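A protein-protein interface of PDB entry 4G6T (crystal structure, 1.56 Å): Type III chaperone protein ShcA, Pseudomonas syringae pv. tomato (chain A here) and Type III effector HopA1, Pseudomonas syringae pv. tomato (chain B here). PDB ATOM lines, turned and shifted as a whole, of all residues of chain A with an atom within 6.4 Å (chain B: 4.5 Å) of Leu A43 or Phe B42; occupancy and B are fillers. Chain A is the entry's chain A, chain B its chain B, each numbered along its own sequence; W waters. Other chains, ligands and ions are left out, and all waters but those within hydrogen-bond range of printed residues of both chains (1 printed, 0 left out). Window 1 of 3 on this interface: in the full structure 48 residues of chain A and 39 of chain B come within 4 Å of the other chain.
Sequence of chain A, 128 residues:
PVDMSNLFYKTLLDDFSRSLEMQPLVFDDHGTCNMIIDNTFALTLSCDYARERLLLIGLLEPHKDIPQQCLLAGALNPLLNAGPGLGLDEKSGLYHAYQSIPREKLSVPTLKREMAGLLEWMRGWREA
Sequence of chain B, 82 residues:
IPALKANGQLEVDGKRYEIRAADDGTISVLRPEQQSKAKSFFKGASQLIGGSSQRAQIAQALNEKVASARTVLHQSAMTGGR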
ATOM      1  N   THR A  32       4.302  15.681 -32.467  1.00  0.00           N
ATOM      2  CA  THR A  32       5.022  14.514 -31.984  1.00  0.00           C
ATOM      3  C   THR A  32       4.289  13.777 -30.903  1.00  0.00           C
ATOM      4  O   THR A  32       3.465  14.358 -30.159  1.00  0.00           O
ATOM      5  CB  THR A  32       6.416  14.863 -31.522  1.00  0.00           C
ATOM      6  OG1 THR A  32       6.384  15.590 -30.282  1.00  0.00           O
ATOM      7  CG2 THR A  32       7.135  15.693 -32.589  1.00  0.00           C
ATOM      8  N   CYS A  33       4.522  12.486 -30.873  1.00  0.00           N
ATOM      9  CA  CYS A  33       3.930  11.586 -29.876  1.00  0.00           C
ATOM     10  C   CYS A  33       5.070  10.798 -29.257  1.00  0.00           C
ATOM     11  O   CYS A  33       5.548   9.854 -29.877  1.00  0.00           O
ATOM     12  CB  CYS A  33       2.925  10.614 -30.495  1.00  0.00           C
ATOM     13  SG  CYS A  33       2.179   9.503 -29.243  1.00  0.00           S
ATOM     14  N   ASN A  34       5.472  11.131 -28.016  1.00  0.00           N
ATOM     15  CA  ASN A  34       6.546  10.459 -27.295  1.00  0.00           C
ATOM     16  C   ASN A  34       6.018   9.295 -26.555  1.00  0.00           C
ATOM     17  O   ASN A  34       4.940   9.424 -25.895  1.00  0.00           O
ATOM     18  CB  ASN A  34       7.181  11.407 -26.290  1.00  0.00           C
ATOM     19  CG  ASN A  34       7.873  12.575 -26.901  1.00  0.00           C
ATOM     20  OD1 ASN A  34       8.261  12.534 -28.076  1.00  0.00           O
ATOM     21  ND2 ASN A  34       8.053  13.632 -26.126  1.00  0.00           N
ATOM     22  N   MET A  35       6.717   8.180 -26.589  1.00  0.00           N
ATOM     23  CA  MET A  35       6.282   6.949 -26.002  1.00  0.00           C
ATOM     24  C   MET A  35       7.474   6.255 -25.320  1.00  0.00           C
ATOM     25  O   MET A  35       8.637   6.408 -25.714  1.00  0.00           O
ATOM     26  CB  MET A  35       5.763   5.989 -27.044  1.00  0.00           C
ATOM     27  CG  MET A  35       4.498   6.430 -27.737  1.00  0.00           C
ATOM     28  SD  MET A  35       4.222   5.309 -29.155  1.00  0.00           S
ATOM     29  CE  MET A  35       5.298   6.140 -30.326  1.00  0.00           C
ATOM     30  N   ILE A  36       7.183   5.504 -24.239  1.00  0.00           N
ATOM     31  CA  ILE A  36       8.120   4.563 -23.671  1.00  0.00           C
ATOM     32  C   ILE A  36       7.617   3.163 -23.870  1.00  0.00           C
ATOM     33  O   ILE A  36       6.448   2.880 -23.595  1.00  0.00           O
ATOM     34  CB  ILE A  36       8.432   4.835 -22.178  1.00  0.00           C
ATOM     35  CG1 ILE A  36       9.106   6.197 -21.996  1.00  0.00           C
ATOM     36  CG2 ILE A  36       9.261   3.673 -21.583  1.00  0.00           C
ATOM     37  CD1 ILE A  36       9.169   6.755 -20.583  1.00  0.00           C
ATOM     38  N   ILE A  37       8.451   2.257 -24.395  1.00  0.00           N
ATOM     39  CA  ILE A  37       8.107   0.905 -24.725  1.00  0.00           C
ATOM     40  C   ILE A  37       8.823  -0.021 -23.784  1.00  0.00           C
ATOM     41  O   ILE A  37      10.022   0.048 -23.614  1.00  0.00           O
ATOM     42  CB  ILE A  37       8.382   0.533 -26.229  1.00  0.00           C
ATOM     43  CG1 ILE A  37       7.365   1.233 -27.119  1.00  0.00           C
ATOM     44  CG2 ILE A  37       8.297  -0.959 -26.454  1.00  0.00           C
ATOM     45  CD1 ILE A  37       7.407   2.700 -27.138  1.00  0.00           C
ATOM     46  N   PHE A  41      12.624   1.451 -23.853  1.00  0.00           N
ATOM     47  CA  PHE A  41      12.992   2.163 -25.058  1.00  0.00           C
ATOM     48  C   PHE A  41      12.229   3.481 -25.164  1.00  0.00           C
ATOM     49  O   PHE A  41      11.004   3.533 -24.925  1.00  0.00           O
ATOM     50  CB  PHE A  41      12.686   1.343 -26.279  1.00  0.00           C
ATOM     51  CG  PHE A  41      13.524   0.137 -26.425  1.00  0.00           C
ATOM     52  CD1 PHE A  41      14.900   0.298 -26.631  1.00  0.00           C
ATOM     53  CD2 PHE A  41      12.978  -1.108 -26.451  1.00  0.00           C
ATOM     54  CE1 PHE A  41      15.698  -0.791 -26.800  1.00  0.00           C
ATOM     55  CE2 PHE A  41      13.787  -2.212 -26.651  1.00  0.00           C
ATOM     56  CZ  PHE A  41      15.152  -2.040 -26.810  1.00  0.00           C
ATOM     57  N   ALA A  42      12.914   4.503 -25.624  1.00  0.00           N
ATOM     58  CA  ALA A  42      12.335   5.770 -25.918  1.00  0.00           C
ATOM     59  C   ALA A  42      12.077   5.947 -27.410  1.00  0.00           C
ATOM     60  O   ALA A  42      13.034   5.819 -28.164  1.00  0.00           O
ATOM     61  CB  ALA A  42      13.192   6.904 -25.382  1.00  0.00           C
ATOM     62  N   LEU A  43      10.840   6.249 -27.804  1.00  0.00           N
ATOM     63  CA  LEU A  43      10.421   6.254 -29.234  1.00  0.00           C
ATOM     64  C   LEU A  43       9.539   7.472 -29.405  1.00  0.00           C
ATOM     65  O   LEU A  43       8.778   7.891 -28.505  1.00  0.00           O
ATOM     66  CB  LEU A  43       9.727   4.964 -29.638  1.00  0.00           C
ATOM     67  CG  LEU A  43       9.551   4.536 -31.112  1.00  0.00           C
ATOM     68  CD1 LEU A  43       9.595   3.030 -31.279  1.00  0.00           C
ATOM     69  CD2 LEU A  43       8.236   5.070 -31.674  1.00  0.00           C
ATOM     70  N   THR A  44       9.625   8.121 -30.550  1.00  0.00           N
ATOM     71  CA  THR A  44       8.764   9.238 -30.867  1.00  0.00           C
ATOM     72  C   THR A  44       8.201   9.062 -32.247  1.00  0.00           C
ATOM     73  O   THR A  44       8.917   8.630 -33.164  1.00  0.00           O
ATOM     74  CB  THR A  44       9.371  10.624 -30.740  1.00  0.00           C
ATOM     75  OG1 THR A  44       9.988  10.743 -29.432  1.00  0.00           O
ATOM     76  CG2 THR A  44       8.205  11.601 -30.790  1.00  0.00           C
ATOM     77  N   LEU A  45       6.921   9.322 -32.414  1.00  0.00           N
ATOM     78  CA  LEU A  45       6.334   9.456 -33.758  1.00  0.00           C
ATOM     79  C   LEU A  45       6.196  10.927 -34.074  1.00  0.00           C
ATOM     80  O   LEU A  45       5.662  11.711 -33.255  1.00  0.00           O
ATOM     81  CB  LEU A  45       4.973   8.829 -33.801  1.00  0.00           C
ATOM     82  CG  LEU A  45       4.782   7.365 -33.563  1.00  0.00           C
ATOM     83  CD1 LEU A  45       3.323   6.952 -33.634  1.00  0.00           C
ATOM     84  CD2 LEU A  45       5.633   6.518 -34.499  1.00  0.00           C
ATOM     85  N   LEU A  56       9.350   7.612 -37.432  1.00  0.00           N
ATOM     86  CA  LEU A  56       9.540   6.838 -36.196  1.00  0.00           C
ATOM     87  C   LEU A  56      10.966   7.080 -35.768  1.00  0.00           C
ATOM     88  O   LEU A  56      11.919   6.817 -36.546  1.00  0.00           O
ATOM     89  CB  LEU A  56       9.311   5.382 -36.444  1.00  0.00           C
ATOM     90  CG  LEU A  56       7.929   4.835 -36.756  1.00  0.00           C
ATOM     91  CD1 LEU A  56       7.154   5.708 -37.751  1.00  0.00           C
ATOM     92  CD2 LEU A  56       7.917   3.406 -37.208  1.00  0.00           C
ATOM     93  N   ILE A  57      11.190   7.558 -34.550  1.00  0.00           N
ATOM     94  CA  ILE A  57      12.496   7.957 -34.099  1.00  0.00           C
ATOM     95  C   ILE A  57      12.761   7.323 -32.760  1.00  0.00           C
ATOM     96  O   ILE A  57      11.884   7.332 -31.880  1.00  0.00           O
ATOM     97  CB  ILE A  57      12.643   9.455 -33.926  1.00  0.00           C
ATOM     98  CG1 ILE A  57      12.114  10.241 -35.167  1.00  0.00           C
ATOM     99  CG2 ILE A  57      14.107   9.862 -33.676  1.00  0.00           C
ATOM    100  CD1 ILE A  57      11.981  11.735 -35.035  1.00  0.00           C
ATOM    101  N   GLY A  58      13.920   6.711 -32.613  1.00  0.00           N
ATOM    102  CA  GLY A  58      14.268   6.035 -31.385  1.00  0.00           C
ATOM    103  C   GLY A  58      15.599   6.434 -30.843  1.00  0.00           C
ATOM    104  O   GLY A  58      16.538   6.733 -31.572  1.00  0.00           O
ATOM    105  N   LEU A  59      15.736   6.398 -29.515  1.00  0.00           N
ATOM    106  CA  LEU A  59      17.025   6.670 -28.832  1.00  0.00           C
ATOM    107  C   LEU A  59      17.880   5.440 -28.862  1.00  0.00           C
ATOM    108  O   LEU A  59      17.508   4.407 -28.371  1.00  0.00           O
ATOM    109  CB  LEU A  59      16.787   7.114 -27.368  1.00  0.00           C
ATOM    110  CG  LEU A  59      18.083   7.241 -26.559  1.00  0.00           C
ATOM    111  CD1 LEU A  59      19.078   8.242 -27.107  1.00  0.00           C
ATOM    112  CD2 LEU A  59      17.726   7.651 -25.091  1.00  0.00           C
ATOM    113  N   MET A 115       7.291  -0.187 -36.345  1.00  0.00           N
ATOM    114  CA  MET A 115       7.695   0.104 -34.974  1.00  0.00           C
ATOM    115  C   MET A 115       8.431  -1.095 -34.408  1.00  0.00           C
ATOM    116  O   MET A 115       9.450  -0.893 -33.775  1.00  0.00           O
ATOM    117  CB  MET A 115       6.446   0.409 -34.185  1.00  0.00           C
ATOM    118  CG  MET A 115       6.055   1.826 -34.347  1.00  0.00           C
ATOM    119  SD  MET A 115       4.599   2.273 -33.352  1.00  0.00           S
ATOM    120  CE  MET A 115       5.304   1.600 -31.793  1.00  0.00           C
ATOM    121  N   LEU A 118      11.940  -1.177 -35.775  1.00  0.00           N
ATOM    122  CA  LEU A 118      12.768  -0.200 -35.201  1.00  0.00           C
ATOM    123  C   LEU A 118      13.228  -0.649 -33.835  1.00  0.00           C
ATOM    124  O   LEU A 118      14.362  -0.402 -33.466  1.00  0.00           O
ATOM    125  CB  LEU A 118      12.042   1.169 -35.117  1.00  0.00           C
ATOM    126  CG  LEU A 118      12.770   2.325 -34.540  1.00  0.00           C
ATOM    127  CD1 LEU A 118      13.973   2.600 -35.400  1.00  0.00           C
ATOM    128  CD2 LEU A 118      11.909   3.539 -34.330  1.00  0.00           C
ATOM    129  N   LEU A 119      12.285  -1.169 -33.041  1.00  0.00           N
ATOM    130  CA  LEU A 119      12.618  -1.611 -31.697  1.00  0.00           C
ATOM    131  C   LEU A 119      13.646  -2.694 -31.714  1.00  0.00           C
ATOM    132  O   LEU A 119      14.541  -2.663 -30.828  1.00  0.00           O
ATOM    133  CB  LEU A 119      11.336  -2.053 -30.950  1.00  0.00           C
ATOM    134  CG  LEU A 119      10.446  -0.866 -30.571  1.00  0.00           C
ATOM    135  CD1 LEU A 119       8.985  -1.331 -30.337  1.00  0.00           C
ATOM    136  CD2 LEU A 119      10.932   0.009 -29.442  1.00  0.00           C
ATOM    137  N   MET A 122      17.016  -1.190 -32.449  1.00  0.00           N
ATOM    138  CA  MET A 122      17.479  -0.553 -31.215  1.00  0.00           C
ATOM    139  C   MET A 122      18.025  -1.607 -30.258  1.00  0.00           C
ATOM    140  O   MET A 122      19.081  -1.408 -29.674  1.00  0.00           O
ATOM    141  CB  MET A 122      16.322   0.232 -30.611  1.00  0.00           C
ATOM    142  CG  MET A 122      16.004   1.477 -31.441  1.00  0.00           C
ATOM    143  SD  MET A 122      14.404   2.194 -31.085  1.00  0.00           S
ATOM    144  CE  MET A 122      14.723   2.804 -29.380  1.00  0.00           C
ATOM    145  N   ALA B  22       4.808   8.900 -22.996  1.00  0.00           N
ATOM    146  CA  ALA B  22       5.903   9.414 -22.248  1.00  0.00           C
ATOM    147  C   ALA B  22       5.730  10.744 -21.569  1.00  0.00           C
ATOM    148  O   ALA B  22       6.476  11.693 -21.798  1.00  0.00           O
ATOM    149  CB  ALA B  22       7.164   9.485 -23.097  1.00  0.00           C
ATOM    150  N   ILE B  27       8.382   8.625 -17.308  1.00  0.00           N
ATOM    151  CA  ILE B  27       9.865   8.689 -17.413  1.00  0.00           C
ATOM    152  C   ILE B  27      10.491   8.274 -16.091  1.00  0.00           C
ATOM    153  O   ILE B  27      11.465   7.501 -16.093  1.00  0.00           O
ATOM    154  CB  ILE B  27      10.332  10.113 -17.832  1.00  0.00           C
ATOM    155  CG1 ILE B  27      10.006  10.331 -19.337  1.00  0.00           C
ATOM    156  CG2 ILE B  27      11.832  10.290 -17.598  1.00  0.00           C
ATOM    157  CD1 ILE B  27       9.782  11.773 -19.842  1.00  0.00           C
ATOM    158  N   ALA B  38      16.977   9.673 -21.869  1.00  0.00           N
ATOM    159  CA  ALA B  38      15.623   9.607 -22.378  1.00  0.00           C
ATOM    160  C   ALA B  38      15.027  10.998 -22.368  1.00  0.00           C
ATOM    161  O   ALA B  38      14.402  11.435 -23.369  1.00  0.00           O
ATOM    162  CB  ALA B  38      14.750   8.653 -21.564  1.00  0.00           C
ATOM    163  N   LYS B  39      15.206  11.735 -21.274  1.00  0.00           N
ATOM    164  CA  LYS B  39      14.693  13.081 -21.193  1.00  0.00           C
ATOM    165  C   LYS B  39      15.284  13.980 -22.280  1.00  0.00           C
ATOM    166  O   LYS B  39      14.537  14.740 -22.922  1.00  0.00           O
ATOM    167  CB  LYS B  39      14.941  13.663 -19.799  1.00  0.00           C
ATOM    168  CG  LYS B  39      14.064  13.011 -18.749  1.00  0.00           C
ATOM    169  CD  LYS B  39      14.213  13.801 -17.439  1.00  0.00           C
ATOM    170  CE  LYS B  39      14.213  12.927 -16.193  1.00  0.00           C
ATOM    171  NZ  LYS B  39      14.633  13.757 -15.025  1.00  0.00           N
ATOM    172  N   SER B  40      16.595  13.872 -22.499  1.00  0.00           N
ATOM    173  CA  SER B  40      17.269  14.692 -23.507  1.00  0.00           C
ATOM    174  C   SER B  40      16.724  14.340 -24.912  1.00  0.00           C
ATOM    175  O   SER B  40      16.465  15.247 -25.741  1.00  0.00           O
ATOM    176  CB  SER B  40      18.755  14.476 -23.504  1.00  0.00           C
ATOM    177  OG  SER B  40      19.332  15.029 -22.334  1.00  0.00           O
ATOM    178  N   PHE B  41      16.573  13.049 -25.167  1.00  0.00           N
ATOM    179  CA  PHE B  41      16.005  12.586 -26.445  1.00  0.00           C
ATOM    180  C   PHE B  41      14.629  13.195 -26.653  1.00  0.00           C
ATOM    181  O   PHE B  41      14.345  13.783 -27.701  1.00  0.00           O
ATOM    182  CB  PHE B  41      15.941  11.087 -26.432  1.00  0.00           C
ATOM    183  CG  PHE B  41      15.146  10.513 -27.551  1.00  0.00           C
ATOM    184  CD1 PHE B  41      15.726  10.394 -28.797  1.00  0.00           C
ATOM    185  CD2 PHE B  41      13.842  10.134 -27.373  1.00  0.00           C
ATOM    186  CE1 PHE B  41      14.998   9.888 -29.836  1.00  0.00           C
ATOM    187  CE2 PHE B  41      13.095   9.639 -28.417  1.00  0.00           C
ATOM    188  CZ  PHE B  41      13.691   9.496 -29.654  1.00  0.00           C
ATOM    189  N   PHE B  42      13.755  13.081 -25.668  1.00  0.00           N
ATOM    190  CA  PHE B  42      12.368  13.574 -25.847  1.00  0.00           C
ATOM    191  C   PHE B  42      12.322  15.081 -26.017  1.00  0.00           C
ATOM    192  O   PHE B  42      11.509  15.631 -26.777  1.00  0.00           O
ATOM    193  CB  PHE B  42      11.448  13.138 -24.697  1.00  0.00           C
ATOM    194  CG  PHE B  42      11.122  11.712 -24.669  1.00  0.00           C
ATOM    195  CD1 PHE B  42      10.649  11.034 -25.804  1.00  0.00           C
ATOM    196  CD2 PHE B  42      11.204  10.993 -23.487  1.00  0.00           C
ATOM    197  CE1 PHE B  42      10.322   9.678 -25.765  1.00  0.00           C
ATOM    198  CE2 PHE B  42      10.835   9.651 -23.435  1.00  0.00           C
ATOM    199  CZ  PHE B  42      10.381   8.976 -24.570  1.00  0.00           C
ATOM    200  N   LYS B  43      13.186  15.784 -25.308  1.00  0.00           N
ATOM    201  CA  LYS B  43      13.225  17.236 -25.373  1.00  0.00           C
ATOM    202  C   LYS B  43      13.594  17.731 -26.750  1.00  0.00           C
ATOM    203  O   LYS B  43      13.078  18.734 -27.190  1.00  0.00           O
ATOM    204  CB  LYS B  43      14.219  17.758 -24.327  1.00  0.00           C
ATOM    205  CG  LYS B  43      14.580  19.232 -24.447  1.00  0.00           C
ATOM    206  CD  LYS B  43      15.052  19.810 -23.112  1.00  0.00           C
ATOM    207  CE  LYS B  43      15.387  21.288 -23.252  1.00  0.00           C
ATOM    208  NZ  LYS B  43      15.903  21.872 -21.986  1.00  0.00           N
ATOM    209  N   GLY B  44      14.534  17.045 -27.389  1.00  0.00           N
ATOM    210  CA  GLY B  44      15.041  17.463 -28.692  1.00  0.00           C
ATOM    211  C   GLY B  44      14.224  16.895 -29.831  1.00  0.00           C
ATOM    212  O   GLY B  44      14.367  17.406 -30.951  1.00  0.00           O
ATOM    213  N   ALA B  45      13.365  15.907 -29.581  1.00  0.00           N
ATOM    214  CA  ALA B  45      12.852  15.078 -30.713  1.00  0.00           C
ATOM    215  C   ALA B  45      12.019  15.903 -31.686  1.00  0.00           C
ATOM    216  O   ALA B  45      12.090  15.702 -32.908  1.00  0.00           O
ATOM    217  CB  ALA B  45      12.060  13.849 -30.233  1.00  0.00           C
HETATM  218  O   HOH W   1       7.903  13.611 -23.314  1.00  0.00           O
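The backbone NH (N) of Ala B22 lies within hydrogen-bond range of the backbone carbonyl oxygen (O) of Asn A34.
N of Leu A59 lies within hydrogen-bond range of O of Ala A42, at 3.1 Å. The backbone NH (N) of Thr A44 is in hydrogen-bond range of the backbone carbonyl oxygen (O) of Ile A57 (2.7 Å). The side-chain amide oxygen (OD1) of Asn A34 is in hydrogen-bond range of the side-chain hydroxyl (OG1) of Thr A44 (2.8 Å). O of Leu A43 is in hydrogen-bond range of N of Met A35, at 2.8 Å.
Among the printed residues, pairs that only touch across the chains: Met A35 with Phe B42 (3.3 Å), Asn A34 with Phe B42 (3.4 Å), Thr A44 with Phe B41 (3.4 Å), Leu A59 with Phe B41 (3.6 Å), Ala A42 with Phe B42 (3.6 Å), Ile A57 with Phe B41 (3.6 Å), Leu A43 with Phe B42 (3.6 Å), Gly A58 with Phe B41 (3.6 Å), Thr A44 with Phe B42 (3.7 Å), Met A35 with Ala B22 (3.8 Å), Ile A36 with Ile B27 (3.8 Å), Thr A44 with Ala B45 (3.8 Å), Ala A42 with Phe B41 (3.8 Å), Leu A59 with Ala B38 (3.9 Å), Ile A36 with Ala B22 (3.97 Å) and Ile A36 with Phe B42 (3.997 Å).
Of the printed residues of chain B, Met A35 touches Ala B22 and Phe B42. Printed residues of chain B within 4 Å of Ala A42: Phe B41 (3.8 Å) and Phe B42 (3.6 Å). Of the printed residues of chain B, Thr A44 touches Phe B41, Phe B42 and Ala B45. Printed residues of chain B within 4 Å of Gly A58: Phe B41 (3.6 Å). Of the printed residues of chain A, Ile B27 touches Ile A36. Lys B43 touches none of the printed residues of chain A.
Of the 19 printed residues of chain A, 9 touch a printed residue of chain B. Hydrophobic or aromatic side chains of chain A within 4 Å of the printed part of chain B: Ile A36, Ala A42, Ile A57 and Leu A59. Of the 10 printed residues of chain B, 6 touch a printed residue of chain A. Printed residues of chain B that touch a printed residue of chain A: Ala B22, Ile B27, Ala B38, Phe B41, Phe B42 and Ala B45. Hydrophobic or aromatic side chains of chain B that line the printed part of chain A: Ala B22, Ile B27, Phe B41, Phe B42 and Ala B45. Along chain B the printed residues that touch a printed residue of chain A span positions 22 to 45. Among the printed residues, no Asp or Glu carboxylate lies within 4 Å of a Lys or Arg side-chain nitrogen of the other chain.
Water W1 lies within hydrogen-bond range of ND2 of Asn A34 (2.8 Å) and O of Ala B22 (2.8 Å).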
